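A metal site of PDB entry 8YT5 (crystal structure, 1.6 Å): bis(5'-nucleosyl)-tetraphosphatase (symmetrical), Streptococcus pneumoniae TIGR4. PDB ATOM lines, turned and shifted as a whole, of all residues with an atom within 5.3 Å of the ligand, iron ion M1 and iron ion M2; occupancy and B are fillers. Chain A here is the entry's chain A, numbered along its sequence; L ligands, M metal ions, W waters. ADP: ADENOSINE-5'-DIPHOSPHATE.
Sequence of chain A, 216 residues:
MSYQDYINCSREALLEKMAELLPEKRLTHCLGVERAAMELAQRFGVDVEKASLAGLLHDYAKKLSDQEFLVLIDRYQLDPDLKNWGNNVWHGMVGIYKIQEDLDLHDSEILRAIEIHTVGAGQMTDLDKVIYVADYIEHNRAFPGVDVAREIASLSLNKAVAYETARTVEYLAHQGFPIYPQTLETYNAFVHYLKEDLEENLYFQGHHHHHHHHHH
OD2 of Asp 59 sits close to NH1 of Arg 26 (3.1 Å). The side-chain hydroxyl (OG1) of Thr 168 sits at hydrogen-bond distance from the backbone carbonyl oxygen (O) of Glu 164. The backbone carbonyl oxygen of Asp 135 sits at hydrogen-bond distance from the guanidinium group of Arg 141 (2.8 Å). A ring nitrogen (ND1) of His 91 lies within hydrogen-bond range of the backbone carbonyl oxygen (O) of Asn 88. The side-chain hydroxyl (OG1) of Thr 118 lies close to a ring nitrogen (NE2) of His 117, at 3.2 Å.
Water W4 lies within hydrogen-bond range of the side-chain carboxylate of Asp 135 (2.6 Å) and an oxygen (O3A) of the ligand (2.9 Å). Water W1 bridges an oxygen (O1B) of the ligand (2.7 Å) and the guanidinium group of Arg 26 (3.2 Å). Water W7 lies within hydrogen-bond range of O of Thr 118 (2.7 Å), N7 of the ligand (2.8 Å) and OG1 of Thr 183 (2.9 Å). Water W6 bridges an oxygen (O1B) of the ligand (2.8 Å) and the guanidinium group of Arg 141 (3.4 Å). Water W11 lies within hydrogen-bond range of O1B of the ligand (3.1 Å) and NZ of Lys 62 (3.3 Å). Water W2 lies within hydrogen-bond range of OD2 of Asp 135, O1A of the ligand and NH1 of Arg 141.
Iron ion M2 is bound by water W4 (1.9 Å), OD1 of Asp 135 (2.0 Å), O2B of the ligand (2.1 Å), NE2 of His 29 (2.1 Å), NE2 of His 58 (2.2 Å) and OD2 of Asp 59 (2.2 Å). Iron ion M2 has six donor atoms within binding distance.
Of the 22 residues printed, 4 come within 4 Å of iron ion M2.
Thr 118 touches iron ion M1 (OG1 to FE, 3.8 Å).
Iron ion M1 is bound by water W4 (2.0 Å), O3B of the ligand (2.0 Å), OD1 of Asp 59 (2.1 Å), NE2 of His 91 (2.2 Å), NE2 of His 117 (2.2 Å) and O2A of the ligand (2.2 Å).
The side-chain hydroxyl of Thr 118 sits close to an oxygen (O2A) of the ligand (2.7 Å). The backbone carbonyl oxygen (O) of Tyr 180 lies close to a nitrogen (N6) of the ligand (3.5 Å). O1B of the ligand lies within salt-bridge range of NZ of Lys 62, 3.1 Å away. An oxygen (O1B) of the ligand is in salt-bridge range of the guanidinium group (NH1) of Arg 26. ND2 of Asn 88 lies close to O4' of the ligand (3.4 Å). A nitrogen (N6) of the ligand lies within hydrogen-bond range of the side-chain hydroxyl (OG1) of Thr 183 (2.7 Å). A nitrogen (N1) of the ligand lies within hydrogen-bond range of the backbone NH (N) of Tyr 180 (3.1 Å).
The backbone carbonyl oxygen (O) of Pro 178 sits close to a nitrogen (N1) of the ligand. Residues that only touch the ligand: Thr 168 (3.8 Å), Leu 172 (3.5 Å) and Ile 179 (3.8 Å). Hydrophobic or aromatic side chains within 4 Å of the ligand: His 29, His 91, His 117, Leu 172, Ile 179 and Tyr 180.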
ATOM      1  N   ARG A  26      -6.286 -29.857  13.452  1.00  0.00           N
ATOM      2  CA  ARG A  26      -5.601 -28.568  13.444  1.00  0.00           C
ATOM      3  C   ARG A  26      -4.326 -28.618  12.601  1.00  0.00           C
ATOM      4  O   ARG A  26      -4.030 -27.652  11.880  1.00  0.00           O
ATOM      5  CB  ARG A  26      -5.319 -28.112  14.883  1.00  0.00           C
ATOM      6  CG  ARG A  26      -4.783 -26.678  15.031  1.00  0.00           C
ATOM      7  CD  ARG A  26      -5.654 -25.607  14.391  1.00  0.00           C
ATOM      8  NE  ARG A  26      -7.024 -25.618  14.893  1.00  0.00           N
ATOM      9  CZ  ARG A  26      -7.971 -24.759  14.528  1.00  0.00           C
ATOM     10  NH1 ARG A  26      -7.711 -23.786  13.659  1.00  0.00           N
ATOM     11  NH2 ARG A  26      -9.194 -24.873  15.035  1.00  0.00           N
ATOM     12  N   HIS A  29      -5.325 -28.598   9.056  1.00  0.00           N
ATOM     13  CA  HIS A  29      -5.648 -27.212   8.700  1.00  0.00           C
ATOM     14  C   HIS A  29      -4.376 -26.422   8.377  1.00  0.00           C
ATOM     15  O   HIS A  29      -4.323 -25.710   7.385  1.00  0.00           O
ATOM     16  CB  HIS A  29      -6.485 -26.554   9.791  1.00  0.00           C
ATOM     17  CG  HIS A  29      -6.494 -25.056   9.749  1.00  0.00           C
ATOM     18  ND1 HIS A  29      -7.187 -24.341   8.800  1.00  0.00           N
ATOM     19  CD2 HIS A  29      -5.912 -24.127  10.558  1.00  0.00           C
ATOM     20  CE1 HIS A  29      -7.022 -23.043   9.014  1.00  0.00           C
ATOM     21  NE2 HIS A  29      -6.263 -22.889  10.077  1.00  0.00           N
ATOM     22  N   VAL A  33      -3.328 -24.494   4.979  1.00  0.00           N
ATOM     23  CA  VAL A  33      -2.936 -23.085   4.915  1.00  0.00           C
ATOM     24  C   VAL A  33      -1.559 -22.934   4.239  1.00  0.00           C
ATOM     25  O   VAL A  33      -1.348 -22.009   3.451  1.00  0.00           O
ATOM     26  CB  VAL A  33      -3.011 -22.406   6.296  1.00  0.00           C
ATOM     27  CG1 VAL A  33      -2.628 -20.943   6.214  1.00  0.00           C
ATOM     28  CG2 VAL A  33      -4.414 -22.517   6.879  1.00  0.00           C
ATOM     29  N   HIS A  58       0.977 -20.701  11.302  1.00  0.00           N
ATOM     30  CA  HIS A  58       0.104 -19.621  11.792  1.00  0.00           C
ATOM     31  C   HIS A  58      -0.686 -20.025  13.045  1.00  0.00           C
ATOM     32  O   HIS A  58      -0.918 -19.193  13.916  1.00  0.00           O
ATOM     33  CB  HIS A  58      -0.823 -19.118  10.692  1.00  0.00           C
ATOM     34  CG  HIS A  58      -2.028 -19.967  10.493  1.00  0.00           C
ATOM     35  ND1 HIS A  58      -1.958 -21.213   9.927  1.00  0.00           N
ATOM     36  CD2 HIS A  58      -3.316 -19.786  10.863  1.00  0.00           C
ATOM     37  CE1 HIS A  58      -3.161 -21.758   9.909  1.00  0.00           C
ATOM     38  NE2 HIS A  58      -4.008 -20.911  10.484  1.00  0.00           N
ATOM     39  N   ASP A  59      -1.081 -21.303  13.141  1.00  0.00           N
ATOM     40  CA  ASP A  59      -1.822 -21.800  14.302  1.00  0.00           C
ATOM     41  C   ASP A  59      -0.984 -22.676  15.225  1.00  0.00           C
ATOM     42  O   ASP A  59      -1.535 -23.445  16.006  1.00  0.00           O
ATOM     43  CB  ASP A  59      -3.107 -22.538  13.874  1.00  0.00           C
ATOM     44  CG  ASP A  59      -4.283 -21.593  13.619  1.00  0.00           C
ATOM     45  OD1 ASP A  59      -4.290 -20.443  14.098  1.00  0.00           O
ATOM     46  OD2 ASP A  59      -5.221 -22.011  12.910  1.00  0.00           O
ATOM     47  N   LYS A  62      -2.083 -22.531  18.875  1.00  0.00           N
ATOM     48  CA  LYS A  62      -3.531 -22.631  19.096  1.00  0.00           C
ATOM     49  C   LYS A  62      -3.912 -23.320  20.410  1.00  0.00           C
ATOM     50  O   LYS A  62      -4.955 -23.010  20.988  1.00  0.00           O
ATOM     51  CB  LYS A  62      -4.192 -23.345  17.921  1.00  0.00           C
ATOM     52  CG  LYS A  62      -5.725 -23.349  17.919  1.00  0.00           C
ATOM     53  CD  LYS A  62      -6.337 -22.018  17.514  1.00  0.00           C
ATOM     54  CE  LYS A  62      -7.834 -22.167  17.273  1.00  0.00           C
ATOM     55  NZ  LYS A  62      -8.442 -20.953  16.640  1.00  0.00           N
ATOM     56  N   TRP A  85      -8.812 -10.503  26.967  1.00  0.00           N
ATOM     57  CA  TRP A  85      -9.304 -11.293  25.845  1.00  0.00           C
ATOM     58  C   TRP A  85      -8.974 -12.763  26.069  1.00  0.00           C
ATOM     59  O   TRP A  85      -8.940 -13.226  27.206  1.00  0.00           O
ATOM     60  CB  TRP A  85      -8.760 -10.721  24.530  1.00  0.00           C
ATOM     61  CG  TRP A  85      -9.162  -9.292  24.390  1.00  0.00           C
ATOM     62  CD1 TRP A  85      -8.499  -8.197  24.862  1.00  0.00           C
ATOM     63  CD2 TRP A  85     -10.367  -8.798  23.773  1.00  0.00           C
ATOM     64  NE1 TRP A  85      -9.190  -7.048  24.569  1.00  0.00           N
ATOM     65  CE2 TRP A  85     -10.347  -7.384  23.908  1.00  0.00           C
ATOM     66  CE3 TRP A  85     -11.438  -9.412  23.117  1.00  0.00           C
ATOM     67  CZ2 TRP A  85     -11.364  -6.567  23.405  1.00  0.00           C
ATOM     68  CZ3 TRP A  85     -12.459  -8.597  22.623  1.00  0.00           C
ATOM     69  CH2 TRP A  85     -12.420  -7.193  22.765  1.00  0.00           C
ATOM     70  N   ASN A  88      -8.559 -16.683  21.023  1.00  0.00           N
ATOM     71  CA  ASN A  88      -8.788 -16.143  19.678  1.00  0.00           C
ATOM     72  C   ASN A  88      -7.816 -15.015  19.330  1.00  0.00           C
ATOM     73  O   ASN A  88      -7.179 -15.052  18.281  1.00  0.00           O
ATOM     74  CB  ASN A  88     -10.233 -15.651  19.496  1.00  0.00           C
ATOM     75  CG  ASN A  88     -11.239 -16.794  19.504  1.00  0.00           C
ATOM     76  OD1 ASN A  88     -10.886 -17.973  19.475  1.00  0.00           O
ATOM     77  ND2 ASN A  88     -12.524 -16.429  19.540  1.00  0.00           N
ATOM     78  N   VAL A  89      -7.680 -14.058  20.230  1.00  0.00           N
ATOM     79  CA  VAL A  89      -6.729 -12.963  20.067  1.00  0.00           C
ATOM     80  C   VAL A  89      -5.305 -13.445  20.318  1.00  0.00           C
ATOM     81  O   VAL A  89      -4.383 -13.126  19.565  1.00  0.00           O
ATOM     82  CB  VAL A  89      -7.096 -11.775  21.000  1.00  0.00           C
ATOM     83  CG1 VAL A  89      -6.036 -10.691  20.939  1.00  0.00           C
ATOM     84  CG2 VAL A  89      -8.440 -11.179  20.614  1.00  0.00           C
ATOM     85  N   HIS A  91      -3.601 -16.411  20.255  1.00  0.00           N
ATOM     86  CA  HIS A  91      -2.783 -17.480  19.643  1.00  0.00           C
ATOM     87  C   HIS A  91      -1.904 -16.955  18.526  1.00  0.00           C
ATOM     88  O   HIS A  91      -0.807 -17.449  18.308  1.00  0.00           O
ATOM     89  CB  HIS A  91      -3.594 -18.716  19.237  1.00  0.00           C
ATOM     90  CG  HIS A  91      -4.455 -18.527  18.029  1.00  0.00           C
ATOM     91  ND1 HIS A  91      -5.628 -17.808  18.060  1.00  0.00           N
ATOM     92  CD2 HIS A  91      -4.311 -18.965  16.761  1.00  0.00           C
ATOM     93  CE1 HIS A  91      -6.166 -17.803  16.856  1.00  0.00           C
ATOM     94  NE2 HIS A  91      -5.395 -18.510  16.048  1.00  0.00           N
ATOM     95  N   HIS A 117      -2.773 -12.733  11.932  1.00  0.00           N
ATOM     96  CA  HIS A 117      -3.536 -13.605  11.019  1.00  0.00           C
ATOM     97  C   HIS A 117      -5.014 -13.714  11.380  1.00  0.00           C
ATOM     98  O   HIS A 117      -5.828 -14.039  10.520  1.00  0.00           O
ATOM     99  CB  HIS A 117      -2.903 -14.993  10.905  1.00  0.00           C
ATOM    100  CG  HIS A 117      -3.300 -15.924  12.018  1.00  0.00           C
ATOM    101  ND1 HIS A 117      -2.533 -16.086  13.144  1.00  0.00           N
ATOM    102  CD2 HIS A 117      -4.374 -16.735  12.160  1.00  0.00           C
ATOM    103  CE1 HIS A 117      -3.123 -16.957  13.948  1.00  0.00           C
ATOM    104  NE2 HIS A 117      -4.233 -17.369  13.374  1.00  0.00           N
ATOM    105  N   THR A 118      -5.362 -13.451  12.639  1.00  0.00           N
ATOM    106  CA  THR A 118      -6.753 -13.529  13.077  1.00  0.00           C
ATOM    107  C   THR A 118      -7.442 -12.181  12.950  1.00  0.00           C
ATOM    108  O   THR A 118      -8.548 -12.098  12.390  1.00  0.00           O
ATOM    109  CB  THR A 118      -6.851 -13.981  14.545  1.00  0.00           C
ATOM    110  OG1 THR A 118      -6.121 -15.194  14.746  1.00  0.00           O
ATOM    111  CG2 THR A 118      -8.314 -14.155  14.979  1.00  0.00           C
ATOM    112  N   VAL A 119      -6.800 -11.124  13.440  1.00  0.00           N
ATOM    113  CA  VAL A 119      -7.445  -9.823  13.557  1.00  0.00           C
ATOM    114  C   VAL A 119      -7.120  -8.834  12.432  1.00  0.00           C
ATOM    115  O   VAL A 119      -7.793  -7.808  12.294  1.00  0.00           O
ATOM    116  CB  VAL A 119      -7.167  -9.176  14.937  1.00  0.00           C
ATOM    117  CG1 VAL A 119      -7.808 -10.006  16.035  1.00  0.00           C
ATOM    118  CG2 VAL A 119      -5.675  -8.991  15.181  1.00  0.00           C
ATOM    119  N   ASP A 135      -5.755 -18.739   5.473  1.00  0.00           N
ATOM    120  CA  ASP A 135      -6.362 -19.334   6.657  1.00  0.00           C
ATOM    121  C   ASP A 135      -7.851 -19.602   6.433  1.00  0.00           C
ATOM    122  O   ASP A 135      -8.389 -20.635   6.847  1.00  0.00           O
ATOM    123  CB  ASP A 135      -6.146 -18.365   7.827  1.00  0.00           C
ATOM    124  CG  ASP A 135      -6.611 -18.900   9.150  1.00  0.00           C
ATOM    125  OD1 ASP A 135      -6.609 -20.133   9.398  1.00  0.00           O
ATOM    126  OD2 ASP A 135      -6.930 -18.051   9.995  1.00  0.00           O
ATOM    127  N   ARG A 141     -11.481 -26.187   4.774  1.00  0.00           N
ATOM    128  CA  ARG A 141     -12.594 -25.346   5.262  1.00  0.00           C
ATOM    129  C   ARG A 141     -13.876 -25.657   4.505  1.00  0.00           C
ATOM    130  O   ARG A 141     -13.857 -25.847   3.298  1.00  0.00           O
ATOM    131  CB  ARG A 141     -12.277 -23.863   5.087  1.00  0.00           C
ATOM    132  CG  ARG A 141     -11.028 -23.322   5.778  1.00  0.00           C
ATOM    133  CD  ARG A 141     -11.031 -23.566   7.266  1.00  0.00           C
ATOM    134  NE  ARG A 141     -12.060 -22.845   7.994  1.00  0.00           N
ATOM    135  CZ  ARG A 141     -11.907 -21.629   8.500  1.00  0.00           C
ATOM    136  NH1 ARG A 141     -10.758 -20.983   8.332  1.00  0.00           N
ATOM    137  NH2 ARG A 141     -12.870 -21.056   9.190  1.00  0.00           N
ATOM    138  N   GLU A 164     -13.566 -11.402   3.938  1.00  0.00           N
ATOM    139  CA  GLU A 164     -13.351 -12.197   5.148  1.00  0.00           C
ATOM    140  C   GLU A 164     -13.645 -11.367   6.400  1.00  0.00           C
ATOM    141  O   GLU A 164     -14.304 -11.847   7.323  1.00  0.00           O
ATOM    142  CB  GLU A 164     -11.932 -12.759   5.207  1.00  0.00           C
ATOM    143  CG  GLU A 164     -11.691 -13.546   6.485  1.00  0.00           C
ATOM    144  CD  GLU A 164     -10.289 -14.097   6.605  1.00  0.00           C
ATOM    145  OE1 GLU A 164      -9.555 -14.088   5.596  1.00  0.00           O
ATOM    146  OE2 GLU A 164      -9.939 -14.562   7.707  1.00  0.00           O
ATOM    147  N   THR A 168     -16.554 -11.925   9.192  1.00  0.00           N
ATOM    148  CA  THR A 168     -16.151 -12.184  10.561  1.00  0.00           C
ATOM    149  C   THR A 168     -16.815 -11.229  11.557  1.00  0.00           C
ATOM    150  O   THR A 168     -17.334 -11.670  12.582  1.00  0.00           O
ATOM    151  CB  THR A 168     -14.628 -12.165  10.683  1.00  0.00           C
ATOM    152  OG1 THR A 168     -14.126 -13.287   9.942  1.00  0.00           O
ATOM    153  CG2 THR A 168     -14.193 -12.304  12.140  1.00  0.00           C
ATOM    154  N   LEU A 172     -19.442 -12.475  14.366  1.00  0.00           N
ATOM    155  CA  LEU A 172     -19.215 -12.244  15.790  1.00  0.00           C
ATOM    156  C   LEU A 172     -20.396 -11.510  16.407  1.00  0.00           C
ATOM    157  O   LEU A 172     -20.855 -11.879  17.493  1.00  0.00           O
ATOM    158  CB  LEU A 172     -17.912 -11.492  16.018  1.00  0.00           C
ATOM    159  CG  LEU A 172     -16.648 -12.276  15.684  1.00  0.00           C
ATOM    160  CD1 LEU A 172     -15.453 -11.352  15.636  1.00  0.00           C
ATOM    161  CD2 LEU A 172     -16.418 -13.424  16.656  1.00  0.00           C
ATOM    162  N   PRO A 178     -17.639 -10.627  21.937  1.00  0.00           N
ATOM    163  CA  PRO A 178     -16.842  -9.400  21.881  1.00  0.00           C
ATOM    164  C   PRO A 178     -15.941  -9.380  20.649  1.00  0.00           C
ATOM    165  O   PRO A 178     -15.461 -10.439  20.197  1.00  0.00           O
ATOM    166  CB  PRO A 178     -15.995  -9.471  23.158  1.00  0.00           C
ATOM    167  CG  PRO A 178     -16.729 -10.397  24.065  1.00  0.00           C
ATOM    168  CD  PRO A 178     -17.357 -11.406  23.157  1.00  0.00           C
ATOM    169  N   ILE A 179     -15.744  -8.193  20.085  1.00  0.00           N
ATOM    170  CA  ILE A 179     -14.927  -8.026  18.894  1.00  0.00           C
ATOM    171  C   ILE A 179     -13.678  -7.238  19.259  1.00  0.00           C
ATOM    172  O   ILE A 179     -13.761  -6.074  19.651  1.00  0.00           O
ATOM    173  CB  ILE A 179     -15.715  -7.316  17.768  1.00  0.00           C
ATOM    174  CG1 ILE A 179     -16.922  -8.170  17.356  1.00  0.00           C
ATOM    175  CG2 ILE A 179     -14.815  -7.022  16.568  1.00  0.00           C
ATOM    176  CD1 ILE A 179     -17.982  -7.414  16.570  1.00  0.00           C
ATOM    177  N   TYR A 180     -12.523  -7.888  19.130  1.00  0.00           N
ATOM    178  CA  TYR A 180     -11.261  -7.212  19.394  1.00  0.00           C
ATOM    179  C   TYR A 180     -11.143  -5.999  18.478  1.00  0.00           C
ATOM    180  O   TYR A 180     -11.352  -6.121  17.280  1.00  0.00           O
ATOM    181  CB  TYR A 180     -10.090  -8.162  19.170  1.00  0.00           C
ATOM    182  CG  TYR A 180      -8.778  -7.623  19.656  1.00  0.00           C
ATOM    183  CD1 TYR A 180      -8.546  -7.439  21.019  1.00  0.00           C
ATOM    184  CD2 TYR A 180      -7.762  -7.297  18.757  1.00  0.00           C
ATOM    185  CE1 TYR A 180      -7.335  -6.933  21.477  1.00  0.00           C
ATOM    186  CE2 TYR A 180      -6.540  -6.797  19.208  1.00  0.00           C
ATOM    187  CZ  TYR A 180      -6.339  -6.625  20.566  1.00  0.00           C
ATOM    188  OH  TYR A 180      -5.135  -6.125  21.019  1.00  0.00           O
ATOM    189  N   THR A 183      -9.669  -5.715  14.810  1.00  0.00           N
ATOM    190  CA  THR A 183     -10.499  -6.211  13.716  1.00  0.00           C
ATOM    191  C   THR A 183     -11.323  -5.122  13.044  1.00  0.00           C
ATOM    192  O   THR A 183     -11.492  -5.114  11.829  1.00  0.00           O
ATOM    193  CB  THR A 183     -11.385  -7.375  14.196  1.00  0.00           C
ATOM    194  OG1 THR A 183     -10.511  -8.463  14.536  1.00  0.00           O
ATOM    195  CG2 THR A 183     -12.382  -7.827  13.146  1.00  0.00           C
HETATM  196  PB  ADP L   1      -8.442 -20.420  13.181  1.00  0.00           P
HETATM  197  O1B ADP L   1      -9.700 -21.003  13.787  1.00  0.00           O
HETATM  198  O2B ADP L   1      -7.948 -21.232  12.011  1.00  0.00           O
HETATM  199  O3B ADP L   1      -7.332 -20.168  14.195  1.00  0.00           O
HETATM  200  PA  ADP L   1      -8.676 -17.506  13.142  1.00  0.00           P
HETATM  201  O1A ADP L   1      -8.843 -16.487  12.034  1.00  0.00           O
HETATM  202  O2A ADP L   1      -7.403 -17.402  13.929  1.00  0.00           O
HETATM  203  O3A ADP L   1      -8.853 -18.994  12.516  1.00  0.00           O
HETATM  204  O5' ADP L   1      -9.905 -17.263  14.136  1.00  0.00           O
HETATM  205  C5' ADP L   1     -10.103 -18.069  15.292  1.00  0.00           C
HETATM  206  C4' ADP L   1     -11.363 -17.570  16.003  1.00  0.00           C
HETATM  207  O4' ADP L   1     -11.181 -16.188  16.382  1.00  0.00           O
HETATM  208  C3' ADP L   1     -12.606 -17.691  15.138  1.00  0.00           C
HETATM  209  O3' ADP L   1     -13.652 -18.309  15.910  1.00  0.00           O
HETATM  210  C2' ADP L   1     -12.911 -16.232  14.890  1.00  0.00           C
HETATM  211  O2' ADP L   1     -14.303 -16.037  14.818  1.00  0.00           O
HETATM  212  C1' ADP L   1     -12.385 -15.522  16.126  1.00  0.00           C
HETATM  213  N9  ADP L   1     -12.161 -14.088  15.934  1.00  0.00           N
HETATM  214  C8  ADP L   1     -11.768 -13.498  14.798  1.00  0.00           C
HETATM  215  N7  ADP L   1     -11.686 -12.168  14.981  1.00  0.00           N
HETATM  216  C5  ADP L   1     -12.028 -11.913  16.241  1.00  0.00           C
HETATM  217  C6  ADP L   1     -12.167 -10.720  17.078  1.00  0.00           C
HETATM  218  N6  ADP L   1     -11.903  -9.488  16.606  1.00  0.00           N
HETATM  219  N1  ADP L   1     -12.561 -10.888  18.347  1.00  0.00           N
HETATM  220  C2  ADP L   1     -12.839 -12.098  18.860  1.00  0.00           C
HETATM  221  N3  ADP L   1     -12.732 -13.226  18.152  1.00  0.00           N
HETATM  222  C4  ADP L   1     -12.344 -13.183  16.860  1.00  0.00           C
HETATM  223 FE    FE M   1      -5.746 -18.913  13.955  1.00  0.00          FE
HETATM  224 FE    FE M   2      -6.071 -21.040  11.122  1.00  0.00          FE
HETATM  225  O   HOH W   1     -11.408 -23.018  13.574  1.00  0.00           O
HETATM  226  O   HOH W   2      -9.938 -18.065   9.453  1.00  0.00           O
HETATM  227  O   HOH W   3     -10.086 -23.096  10.710  1.00  0.00           O
HETATM  228  O   HOH W   4      -6.012 -19.342  12.051  1.00  0.00           O
HETATM  229  O   HOH W   5     -15.069 -15.211  19.800  1.00  0.00           O
HETATM  230  O   HOH W   6     -11.950 -20.118  12.365  1.00  0.00           O
HETATM  231  O   HOH W   7     -10.862 -10.768  12.760  1.00  0.00           O
HETATM  232  O   HOH W   8      -7.943 -15.396   9.433  1.00  0.00           O
HETATM  233  O   HOH W   9     -15.640 -16.933  17.741  1.00  0.00           O
HETATM  234  O   HOH W  10     -14.810 -12.867  21.276  1.00  0.00           O
HETATM  235  O   HOH W  11     -11.620 -21.626  16.094  1.00  0.00           O
